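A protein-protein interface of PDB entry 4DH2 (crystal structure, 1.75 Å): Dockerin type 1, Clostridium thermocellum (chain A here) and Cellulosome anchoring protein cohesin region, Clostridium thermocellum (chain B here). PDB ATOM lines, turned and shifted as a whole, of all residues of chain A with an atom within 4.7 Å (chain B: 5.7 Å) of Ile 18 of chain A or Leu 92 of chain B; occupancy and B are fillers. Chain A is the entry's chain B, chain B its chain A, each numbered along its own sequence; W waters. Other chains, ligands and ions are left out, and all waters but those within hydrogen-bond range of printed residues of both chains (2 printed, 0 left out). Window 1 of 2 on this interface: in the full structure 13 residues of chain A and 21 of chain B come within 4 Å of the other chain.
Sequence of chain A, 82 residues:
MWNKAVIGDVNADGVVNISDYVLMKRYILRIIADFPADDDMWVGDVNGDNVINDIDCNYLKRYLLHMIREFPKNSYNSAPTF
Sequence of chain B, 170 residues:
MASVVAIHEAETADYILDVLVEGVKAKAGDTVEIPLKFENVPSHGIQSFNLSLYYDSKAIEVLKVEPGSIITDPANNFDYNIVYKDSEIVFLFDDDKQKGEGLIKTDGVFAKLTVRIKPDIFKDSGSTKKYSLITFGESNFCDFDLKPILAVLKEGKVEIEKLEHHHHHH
Hydrophobic or aromatic side chains of chain B that line the printed part of chain A: Val 90 and Leu 92. Among the printed residues, Asp or Glu carboxylates within 4 Å of a Lys or Arg side-chain nitrogen of the other chain: Lys 61 of chain A with Asp 79 of chain B.
Among the printed residues, merely in contact across the chains: Leu 64 of chain A with Val 90 of chain B, Ile 18 of chain A with Asn 50 of chain B, Val 22 of chain A with Asp 94 of chain B, Ile 18 of chain A with Ser 48 of chain B, Ile 18 of chain A with Asn 140 of chain B, Leu 65 of chain A with Leu 92 of chain B, Leu 65 of chain A with Val 90 of chain B, Ile 18 of chain A with Phe 141 of chain B, Ile 18 of chain A with Cys 142 of chain B, Leu 65 of chain A with Asp 79 of chain B, Leu 65 of chain A with Tyr 80 of chain B, Val 22 of chain A with Ser 48 of chain B, Lys 61 of chain A with Leu 92 of chain B, Tyr 21 of chain A with Leu 92 of chain B, Tyr 21 of chain A with Asp 94 of chain B, Ile 18 of chain A with Leu 92 of chain B and Ile 18 of chain A with Phe 49 of chain B.
Of the printed residues of chain B, Ile 18 of chain A touches Ser 48, Phe 49, Asn 50, Leu 92, Asn 140, Phe 141 and Cys 142. Asp 20 of chain A touches none of the printed residues of chain B. Of the printed residues of chain A, Ser 48 of chain B touches Ile 18 and Val 22. Printed residues of chain A within 4 Å of Asn 50 of chain B: Ile 18 (3.3 Å) and Leu 64 (3.0 Å). Leu 92 of chain B touches just these residues of chain A: Ile 18 (3.97 Å), Tyr 21 (3.8 Å), Lys 61 (3.8 Å) and Leu 65 (3.6 Å). Of the printed residues of chain A, Phe 141 of chain B touches Ile 18 (3.6 Å). The nearest printed residue of chain B that does not touch Ile 18 of chain A is Phe 93 of chain B (5.4 Å). The nearest residue of chain A that does not touch Leu 92 of chain B is Leu 64 of chain A (4.1 Å). The nearest printed residue of chain A that does not touch Asn 50 of chain B is Leu 65 of chain A (4.9 Å).
OG of Ser 48 of chain B sits at hydrogen-bond distance from O of Phe 93 of chain B (2.8 Å). The backbone NH (N) of Cys 142 of chain B is in hydrogen-bond range of the backbone carbonyl oxygen (O) of Ser 48 of chain B, at 3.0 Å. O of Phe 49 of chain B lies within hydrogen-bond range of N of Phe 93 of chain B (2.9 Å). ND2 of Asn 50 of chain B sits at hydrogen-bond distance from O of Phe 91 of chain B, 2.9 Å away. The backbone carbonyl oxygen (O) of Asn 77 of chain B sits at hydrogen-bond distance from the backbone NH (N) of Asp 94 of chain B (2.9 Å). The backbone carbonyl oxygen (O) of Leu 92 of chain B is in hydrogen-bond range of the backbone NH (N) of Asp 79 of chain B (2.9 Å).
The backbone carbonyl oxygen (O) of Leu 64 of chain A sits at hydrogen-bond distance from the side-chain amide nitrogen (ND2) of Asn 50 of chain B, 3.0 Å away. OD2 of Asp 79 of chain B is in salt-bridge range of NZ of Lys 61 of chain A (2.8 Å).
Water W2 lies within hydrogen-bond range of the side-chain amide oxygen of Asn 50 of chain B (2.8 Å), the side-chain amide nitrogen of Asn 140 of chain B (2.9 Å) and the backbone NH of Ile 18 of chain A (3.2 Å). Water W1 bridges the side-chain amide oxygen (OD1) of Asn 50 of chain B (2.8 Å) and the backbone carbonyl oxygen (O) of Leu 64 of chain A (3.3 Å).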
ATOM      1  N   ASN A  17     -14.119  -0.477   3.296  1.00  0.00           N
ATOM      2  CA  ASN A  17     -15.157  -1.477   3.383  1.00  0.00           C
ATOM      3  C   ASN A  17     -16.443  -0.943   2.754  1.00  0.00           C
ATOM      4  O   ASN A  17     -16.423   0.077   2.029  1.00  0.00           O
ATOM      5  CB  ASN A  17     -15.400  -1.924   4.846  1.00  0.00           C
ATOM      6  CG  ASN A  17     -15.857  -0.797   5.753  1.00  0.00           C
ATOM      7  OD1 ASN A  17     -16.348   0.232   5.290  1.00  0.00           O
ATOM      8  ND2 ASN A  17     -15.679  -0.974   7.084  1.00  0.00           N
ATOM      9  N   ILE A  18     -17.549  -1.639   2.986  1.00  0.00           N
ATOM     10  CA  ILE A  18     -18.778  -1.287   2.307  1.00  0.00           C
ATOM     11  C   ILE A  18     -19.179   0.167   2.548  1.00  0.00           C
ATOM     12  O   ILE A  18     -19.800   0.777   1.691  1.00  0.00           O
ATOM     13  CB  ILE A  18     -19.972  -2.184   2.723  1.00  0.00           C
ATOM     14  CG1 ILE A  18     -20.116  -2.173   4.251  1.00  0.00           C
ATOM     15  CG2 ILE A  18     -19.777  -3.581   2.168  1.00  0.00           C
ATOM     16  CD1 ILE A  18     -21.314  -2.863   4.752  1.00  0.00           C
ATOM     17  N   SER A  19     -18.885   0.734   3.719  1.00  0.00           N
ATOM     18  CA  SER A  19     -19.286   2.118   3.922  1.00  0.00           C
ATOM     19  C   SER A  19     -18.630   3.053   2.899  1.00  0.00           C
ATOM     20  O   SER A  19     -19.245   4.035   2.449  1.00  0.00           O
ATOM     21  CB  SER A  19     -19.001   2.592   5.353  1.00  0.00           C
ATOM     22  OG  SER A  19     -19.821   1.871   6.262  1.00  0.00           O
ATOM     23  N   ASP A  20     -17.372   2.798   2.561  1.00  0.00           N
ATOM     24  CA  ASP A  20     -16.701   3.621   1.569  1.00  0.00           C
ATOM     25  C   ASP A  20     -17.321   3.442   0.196  1.00  0.00           C
ATOM     26  O   ASP A  20     -17.399   4.377  -0.597  1.00  0.00           O
ATOM     27  CB  ASP A  20     -15.236   3.261   1.518  1.00  0.00           C
ATOM     28  CG  ASP A  20     -14.579   3.440   2.873  1.00  0.00           C
ATOM     29  OD1 ASP A  20     -14.408   4.590   3.306  1.00  0.00           O
ATOM     30  OD2 ASP A  20     -14.310   2.408   3.504  1.00  0.00           O
ATOM     31  N   TYR A  21     -17.748   2.223  -0.096  1.00  0.00           N
ATOM     32  CA  TYR A  21     -18.421   1.941  -1.366  1.00  0.00           C
ATOM     33  C   TYR A  21     -19.756   2.683  -1.487  1.00  0.00           C
ATOM     34  O   TYR A  21     -20.060   3.319  -2.517  1.00  0.00           O
ATOM     35  CB  TYR A  21     -18.663   0.431  -1.471  1.00  0.00           C
ATOM     36  CG  TYR A  21     -19.210  -0.062  -2.792  1.00  0.00           C
ATOM     37  CD1 TYR A  21     -18.553   0.200  -3.982  1.00  0.00           C
ATOM     38  CD2 TYR A  21     -20.362  -0.837  -2.832  1.00  0.00           C
ATOM     39  CE1 TYR A  21     -19.047  -0.254  -5.178  1.00  0.00           C
ATOM     40  CE2 TYR A  21     -20.865  -1.302  -4.038  1.00  0.00           C
ATOM     41  CZ  TYR A  21     -20.189  -0.998  -5.201  1.00  0.00           C
ATOM     42  OH  TYR A  21     -20.660  -1.448  -6.411  1.00  0.00           O
ATOM     43  N   VAL A  22     -20.572   2.595  -0.447  1.00  0.00           N
ATOM     44  CA  VAL A  22     -21.852   3.293  -0.434  1.00  0.00           C
ATOM     45  C   VAL A  22     -21.644   4.800  -0.530  1.00  0.00           C
ATOM     46  O   VAL A  22     -22.335   5.489  -1.325  1.00  0.00           O
ATOM     47  CB  VAL A  22     -22.628   2.955   0.850  1.00  0.00           C
ATOM     48  CG1 VAL A  22     -23.880   3.777   0.941  1.00  0.00           C
ATOM     49  CG2 VAL A  22     -22.983   1.434   0.863  1.00  0.00           C
ATOM     50  N   LYS A  61     -15.515  -1.836  -5.921  1.00  0.00           N
ATOM     51  CA  LYS A  61     -16.277  -3.077  -6.008  1.00  0.00           C
ATOM     52  C   LYS A  61     -15.309  -4.237  -6.175  1.00  0.00           C
ATOM     53  O   LYS A  61     -15.415  -5.235  -5.457  1.00  0.00           O
ATOM     54  CB  LYS A  61     -17.268  -3.028  -7.171  1.00  0.00           C
ATOM     55  CG  LYS A  61     -18.041  -4.316  -7.428  1.00  0.00           C
ATOM     56  CD  LYS A  61     -18.870  -4.302  -8.723  1.00  0.00           C
ATOM     57  CE  LYS A  61     -20.174  -3.523  -8.556  1.00  0.00           C
ATOM     58  NZ  LYS A  61     -21.255  -3.869  -9.556  1.00  0.00           N
ATOM     59  N   LEU A  64     -13.528  -5.002  -2.985  1.00  0.00           N
ATOM     60  CA  LEU A  64     -14.349  -5.606  -1.945  1.00  0.00           C
ATOM     61  C   LEU A  64     -14.716  -7.056  -2.314  1.00  0.00           C
ATOM     62  O   LEU A  64     -15.035  -7.851  -1.429  1.00  0.00           O
ATOM     63  CB  LEU A  64     -15.601  -4.781  -1.664  1.00  0.00           C
ATOM     64  CG  LEU A  64     -15.325  -3.423  -1.022  1.00  0.00           C
ATOM     65  CD1 LEU A  64     -16.641  -2.669  -0.891  1.00  0.00           C
ATOM     66  CD2 LEU A  64     -14.618  -3.560   0.348  1.00  0.00           C
ATOM     67  N   LEU A  65     -14.682  -7.358  -3.611  1.00  0.00           N
ATOM     68  CA  LEU A  65     -14.921  -8.709  -4.110  1.00  0.00           C
ATOM     69  C   LEU A  65     -13.617  -9.532  -4.118  1.00  0.00           C
ATOM     70  O   LEU A  65     -13.620 -10.684  -4.550  1.00  0.00           O
ATOM     71  CB  LEU A  65     -15.507  -8.657  -5.522  1.00  0.00           C
ATOM     72  CG  LEU A  65     -17.006  -8.267  -5.660  1.00  0.00           C
ATOM     73  CD1 LEU A  65     -17.399  -8.065  -7.103  1.00  0.00           C
ATOM     74  CD2 LEU A  65     -17.954  -9.284  -4.996  1.00  0.00           C
ATOM     75  N   SER B  48     -26.263  -2.529   2.450  1.00  0.00           N
ATOM     76  CA  SER B  48     -25.134  -3.153   1.798  1.00  0.00           C
ATOM     77  C   SER B  48     -24.539  -4.246   2.687  1.00  0.00           C
ATOM     78  O   SER B  48     -24.560  -4.131   3.921  1.00  0.00           O
ATOM     79  CB  SER B  48     -24.055  -2.126   1.514  1.00  0.00           C
ATOM     80  OG  SER B  48     -22.897  -2.721   0.933  1.00  0.00           O
ATOM     81  N   PHE B  49     -23.986  -5.267   2.050  1.00  0.00           N
ATOM     82  CA  PHE B  49     -23.203  -6.245   2.799  1.00  0.00           C
ATOM     83  C   PHE B  49     -22.119  -6.815   1.953  1.00  0.00           C
ATOM     84  O   PHE B  49     -22.201  -6.823   0.721  1.00  0.00           O
ATOM     85  CB  PHE B  49     -24.079  -7.358   3.397  1.00  0.00           C
ATOM     86  CG  PHE B  49     -24.656  -8.342   2.379  1.00  0.00           C
ATOM     87  CD1 PHE B  49     -23.894  -9.377   1.862  1.00  0.00           C
ATOM     88  CD2 PHE B  49     -25.974  -8.228   1.977  1.00  0.00           C
ATOM     89  CE1 PHE B  49     -24.450 -10.275   0.978  1.00  0.00           C
ATOM     90  CE2 PHE B  49     -26.528  -9.104   1.095  1.00  0.00           C
ATOM     91  CZ  PHE B  49     -25.764 -10.137   0.584  1.00  0.00           C
ATOM     92  N   ASN B  50     -21.075  -7.292   2.624  1.00  0.00           N
ATOM     93  CA  ASN B  50     -19.919  -7.879   1.973  1.00  0.00           C
ATOM     94  C   ASN B  50     -19.552  -9.030   2.895  1.00  0.00           C
ATOM     95  O   ASN B  50     -19.332  -8.821   4.107  1.00  0.00           O
ATOM     96  CB  ASN B  50     -18.874  -6.771   1.884  1.00  0.00           C
ATOM     97  CG  ASN B  50     -17.564  -7.148   1.198  1.00  0.00           C
ATOM     98  OD1 ASN B  50     -16.553  -6.544   1.536  1.00  0.00           O
ATOM     99  ND2 ASN B  50     -17.562  -8.076   0.235  1.00  0.00           N
ATOM    100  N   LEU B  51     -19.536 -10.241   2.330  1.00  0.00           N
ATOM    101  CA  LEU B  51     -19.422 -11.475   3.117  1.00  0.00           C
ATOM    102  C   LEU B  51     -18.533 -12.446   2.329  1.00  0.00           C
ATOM    103  O   LEU B  51     -18.670 -12.514   1.099  1.00  0.00           O
ATOM    104  CB  LEU B  51     -20.841 -12.055   3.282  1.00  0.00           C
ATOM    105  CG  LEU B  51     -21.069 -13.391   3.966  1.00  0.00           C
ATOM    106  CD1 LEU B  51     -20.464 -13.347   5.316  1.00  0.00           C
ATOM    107  CD2 LEU B  51     -22.555 -13.580   4.074  1.00  0.00           C
ATOM    108  N   ASN B  77     -27.597  -4.853  -8.089  1.00  0.00           N
ATOM    109  CA  ASN B  77     -27.293  -4.750  -6.649  1.00  0.00           C
ATOM    110  C   ASN B  77     -26.401  -5.857  -6.089  1.00  0.00           C
ATOM    111  O   ASN B  77     -25.900  -5.733  -4.965  1.00  0.00           O
ATOM    112  CB  ASN B  77     -28.573  -4.731  -5.845  1.00  0.00           C
ATOM    113  CG  ASN B  77     -29.380  -3.484  -6.050  1.00  0.00           C
ATOM    114  OD1 ASN B  77     -28.977  -2.523  -6.719  1.00  0.00           O
ATOM    115  ND2 ASN B  77     -30.532  -3.494  -5.465  1.00  0.00           N
ATOM    116  N   PHE B  78     -26.199  -6.911  -6.873  1.00  0.00           N
ATOM    117  CA  PHE B  78     -25.592  -8.160  -6.379  1.00  0.00           C
ATOM    118  C   PHE B  78     -24.427  -8.599  -7.255  1.00  0.00           C
ATOM    119  O   PHE B  78     -24.550  -8.689  -8.479  1.00  0.00           O
ATOM    120  CB  PHE B  78     -26.662  -9.258  -6.282  1.00  0.00           C
ATOM    121  CG  PHE B  78     -26.143 -10.570  -5.793  1.00  0.00           C
ATOM    122  CD1 PHE B  78     -26.252 -10.908  -4.454  1.00  0.00           C
ATOM    123  CD2 PHE B  78     -25.570 -11.491  -6.669  1.00  0.00           C
ATOM    124  CE1 PHE B  78     -25.780 -12.134  -3.994  1.00  0.00           C
ATOM    125  CE2 PHE B  78     -25.090 -12.713  -6.208  1.00  0.00           C
ATOM    126  CZ  PHE B  78     -25.189 -13.036  -4.880  1.00  0.00           C
ATOM    127  N   ASP B  79     -23.279  -8.816  -6.621  1.00  0.00           N
ATOM    128  CA  ASP B  79     -22.113  -9.351  -7.296  1.00  0.00           C
ATOM    129  C   ASP B  79     -21.474 -10.416  -6.438  1.00  0.00           C
ATOM    130  O   ASP B  79     -21.631 -10.428  -5.217  1.00  0.00           O
ATOM    131  CB  ASP B  79     -21.069  -8.279  -7.510  1.00  0.00           C
ATOM    132  CG  ASP B  79     -21.452  -7.306  -8.601  1.00  0.00           C
ATOM    133  OD1 ASP B  79     -21.242  -7.638  -9.783  1.00  0.00           O
ATOM    134  OD2 ASP B  79     -21.960  -6.216  -8.259  1.00  0.00           O
ATOM    135  N   TYR B  80     -20.727 -11.294  -7.080  1.00  0.00           N
ATOM    136  CA  TYR B  80     -19.888 -12.228  -6.342  1.00  0.00           C
ATOM    137  C   TYR B  80     -18.616 -12.455  -7.118  1.00  0.00           C
ATOM    138  O   TYR B  80     -18.554 -12.190  -8.313  1.00  0.00           O
ATOM    139  CB  TYR B  80     -20.607 -13.553  -6.165  1.00  0.00           C
ATOM    140  CG  TYR B  80     -20.623 -14.362  -7.433  1.00  0.00           C
ATOM    141  CD1 TYR B  80     -19.614 -15.292  -7.698  1.00  0.00           C
ATOM    142  CD2 TYR B  80     -21.621 -14.170  -8.386  1.00  0.00           C
ATOM    143  CE1 TYR B  80     -19.616 -16.021  -8.878  1.00  0.00           C
ATOM    144  CE2 TYR B  80     -21.623 -14.908  -9.581  1.00  0.00           C
ATOM    145  CZ  TYR B  80     -20.620 -15.821  -9.810  1.00  0.00           C
ATOM    146  OH  TYR B  80     -20.621 -16.540 -10.993  1.00  0.00           O
ATOM    147  N   VAL B  90     -16.755 -14.576  -2.453  1.00  0.00           N
ATOM    148  CA  VAL B  90     -17.003 -13.252  -1.890  1.00  0.00           C
ATOM    149  C   VAL B  90     -18.287 -12.692  -2.499  1.00  0.00           C
ATOM    150  O   VAL B  90     -18.511 -12.785  -3.711  1.00  0.00           O
ATOM    151  CB  VAL B  90     -15.833 -12.292  -2.161  1.00  0.00           C
ATOM    152  CG1 VAL B  90     -15.985 -11.026  -1.347  1.00  0.00           C
ATOM    153  CG2 VAL B  90     -14.519 -12.971  -1.807  1.00  0.00           C
ATOM    154  N   PHE B  91     -19.137 -12.141  -1.644  1.00  0.00           N
ATOM    155  CA  PHE B  91     -20.389 -11.537  -2.072  1.00  0.00           C
ATOM    156  C   PHE B  91     -20.353 -10.047  -1.762  1.00  0.00           C
ATOM    157  O   PHE B  91     -19.820  -9.630  -0.739  1.00  0.00           O
ATOM    158  CB  PHE B  91     -21.562 -12.120  -1.292  1.00  0.00           C
ATOM    159  CG  PHE B  91     -21.730 -13.589  -1.456  1.00  0.00           C
ATOM    160  CD1 PHE B  91     -22.550 -14.082  -2.454  1.00  0.00           C
ATOM    161  CD2 PHE B  91     -21.093 -14.471  -0.619  1.00  0.00           C
ATOM    162  CE1 PHE B  91     -22.716 -15.454  -2.616  1.00  0.00           C
ATOM    163  CE2 PHE B  91     -21.267 -15.843  -0.776  1.00  0.00           C
ATOM    164  CZ  PHE B  91     -22.093 -16.311  -1.780  1.00  0.00           C
ATOM    165  N   LEU B  92     -20.934  -9.254  -2.658  1.00  0.00           N
ATOM    166  CA  LEU B  92     -21.147  -7.844  -2.407  1.00  0.00           C
ATOM    167  C   LEU B  92     -22.552  -7.459  -2.849  1.00  0.00           C
ATOM    168  O   LEU B  92     -22.953  -7.661  -4.020  1.00  0.00           O
ATOM    169  CB  LEU B  92     -20.115  -7.027  -3.155  1.00  0.00           C
ATOM    170  CG  LEU B  92     -20.264  -5.518  -2.927  1.00  0.00           C
ATOM    171  CD1 LEU B  92     -19.906  -5.128  -1.483  1.00  0.00           C
ATOM    172  CD2 LEU B  92     -19.372  -4.799  -3.918  1.00  0.00           C
ATOM    173  N   PHE B  93     -23.295  -6.870  -1.919  1.00  0.00           N
ATOM    174  CA  PHE B  93     -24.618  -6.345  -2.207  1.00  0.00           C
ATOM    175  C   PHE B  93     -24.680  -4.889  -1.839  1.00  0.00           C
ATOM    176  O   PHE B  93     -24.149  -4.491  -0.806  1.00  0.00           O
ATOM    177  CB  PHE B  93     -25.664  -7.091  -1.382  1.00  0.00           C
ATOM    178  CG  PHE B  93     -27.004  -6.436  -1.415  1.00  0.00           C
ATOM    179  CD1 PHE B  93     -27.891  -6.699  -2.441  1.00  0.00           C
ATOM    180  CD2 PHE B  93     -27.355  -5.517  -0.451  1.00  0.00           C
ATOM    181  CE1 PHE B  93     -29.124  -6.050  -2.504  1.00  0.00           C
ATOM    182  CE2 PHE B  93     -28.579  -4.850  -0.501  1.00  0.00           C
ATOM    183  CZ  PHE B  93     -29.474  -5.120  -1.543  1.00  0.00           C
ATOM    184  N   ASP B  94     -25.326  -4.083  -2.685  1.00  0.00           N
ATOM    185  CA  ASP B  94     -25.609  -2.711  -2.359  1.00  0.00           C
ATOM    186  C   ASP B  94     -26.880  -2.313  -3.111  1.00  0.00           C
ATOM    187  O   ASP B  94     -27.009  -2.590  -4.297  1.00  0.00           O
ATOM    188  CB  ASP B  94     -24.469  -1.802  -2.808  1.00  0.00           C
ATOM    189  CG  ASP B  94     -24.776  -0.337  -2.634  1.00  0.00           C
ATOM    190  OD1 ASP B  94     -25.071   0.070  -1.490  1.00  0.00           O
ATOM    191  OD2 ASP B  94     -24.736   0.437  -3.648  1.00  0.00           O
ATOM    192  N   ASN B 140     -19.422  -7.838   6.741  1.00  0.00           N
ATOM    193  CA  ASN B 140     -19.723  -6.449   7.042  1.00  0.00           C
ATOM    194  C   ASN B 140     -21.106  -6.119   6.475  1.00  0.00           C
ATOM    195  O   ASN B 140     -21.353  -6.373   5.291  1.00  0.00           O
ATOM    196  CB  ASN B 140     -18.725  -5.524   6.363  1.00  0.00           C
ATOM    197  CG  ASN B 140     -17.390  -5.497   7.045  1.00  0.00           C
ATOM    198  OD1 ASN B 140     -17.298  -5.272   8.260  1.00  0.00           O
ATOM    199  ND2 ASN B 140     -16.331  -5.701   6.266  1.00  0.00           N
ATOM    200  N   PHE B 141     -21.997  -5.586   7.314  1.00  0.00           N
ATOM    201  CA  PHE B 141     -23.346  -5.201   6.883  1.00  0.00           C
ATOM    202  C   PHE B 141     -23.629  -3.802   7.407  1.00  0.00           C
ATOM    203  O   PHE B 141     -23.187  -3.448   8.495  1.00  0.00           O
ATOM    204  CB  PHE B 141     -24.417  -6.098   7.505  1.00  0.00           C
ATOM    205  CG  PHE B 141     -24.447  -7.513   7.001  1.00  0.00           C
ATOM    206  CD1 PHE B 141     -25.551  -8.004   6.337  1.00  0.00           C
ATOM    207  CD2 PHE B 141     -23.394  -8.367   7.247  1.00  0.00           C
ATOM    208  CE1 PHE B 141     -25.589  -9.284   5.887  1.00  0.00           C
ATOM    209  CE2 PHE B 141     -23.448  -9.675   6.817  1.00  0.00           C
ATOM    210  CZ  PHE B 141     -24.525 -10.128   6.133  1.00  0.00           C
ATOM    211  N   CYS B 142     -24.414  -3.020   6.683  1.00  0.00           N
ATOM    212  CA  CYS B 142     -24.853  -1.741   7.212  1.00  0.00           C
ATOM    213  C   CYS B 142     -26.251  -1.375   6.733  1.00  0.00           C
ATOM    214  O   CYS B 142     -26.785  -1.964   5.763  1.00  0.00           O
ATOM    215  CB  CYS B 142     -23.877  -0.620   6.889  1.00  0.00           C
ATOM    216  SG  CYS B 142     -23.866  -0.082   5.113  1.00  0.00           S
HETATM  217  O   HOH W   1     -13.900  -7.407   1.646  1.00  0.00           O
HETATM  218  O   HOH W   2     -16.480  -4.642   3.535  1.00  0.00           O
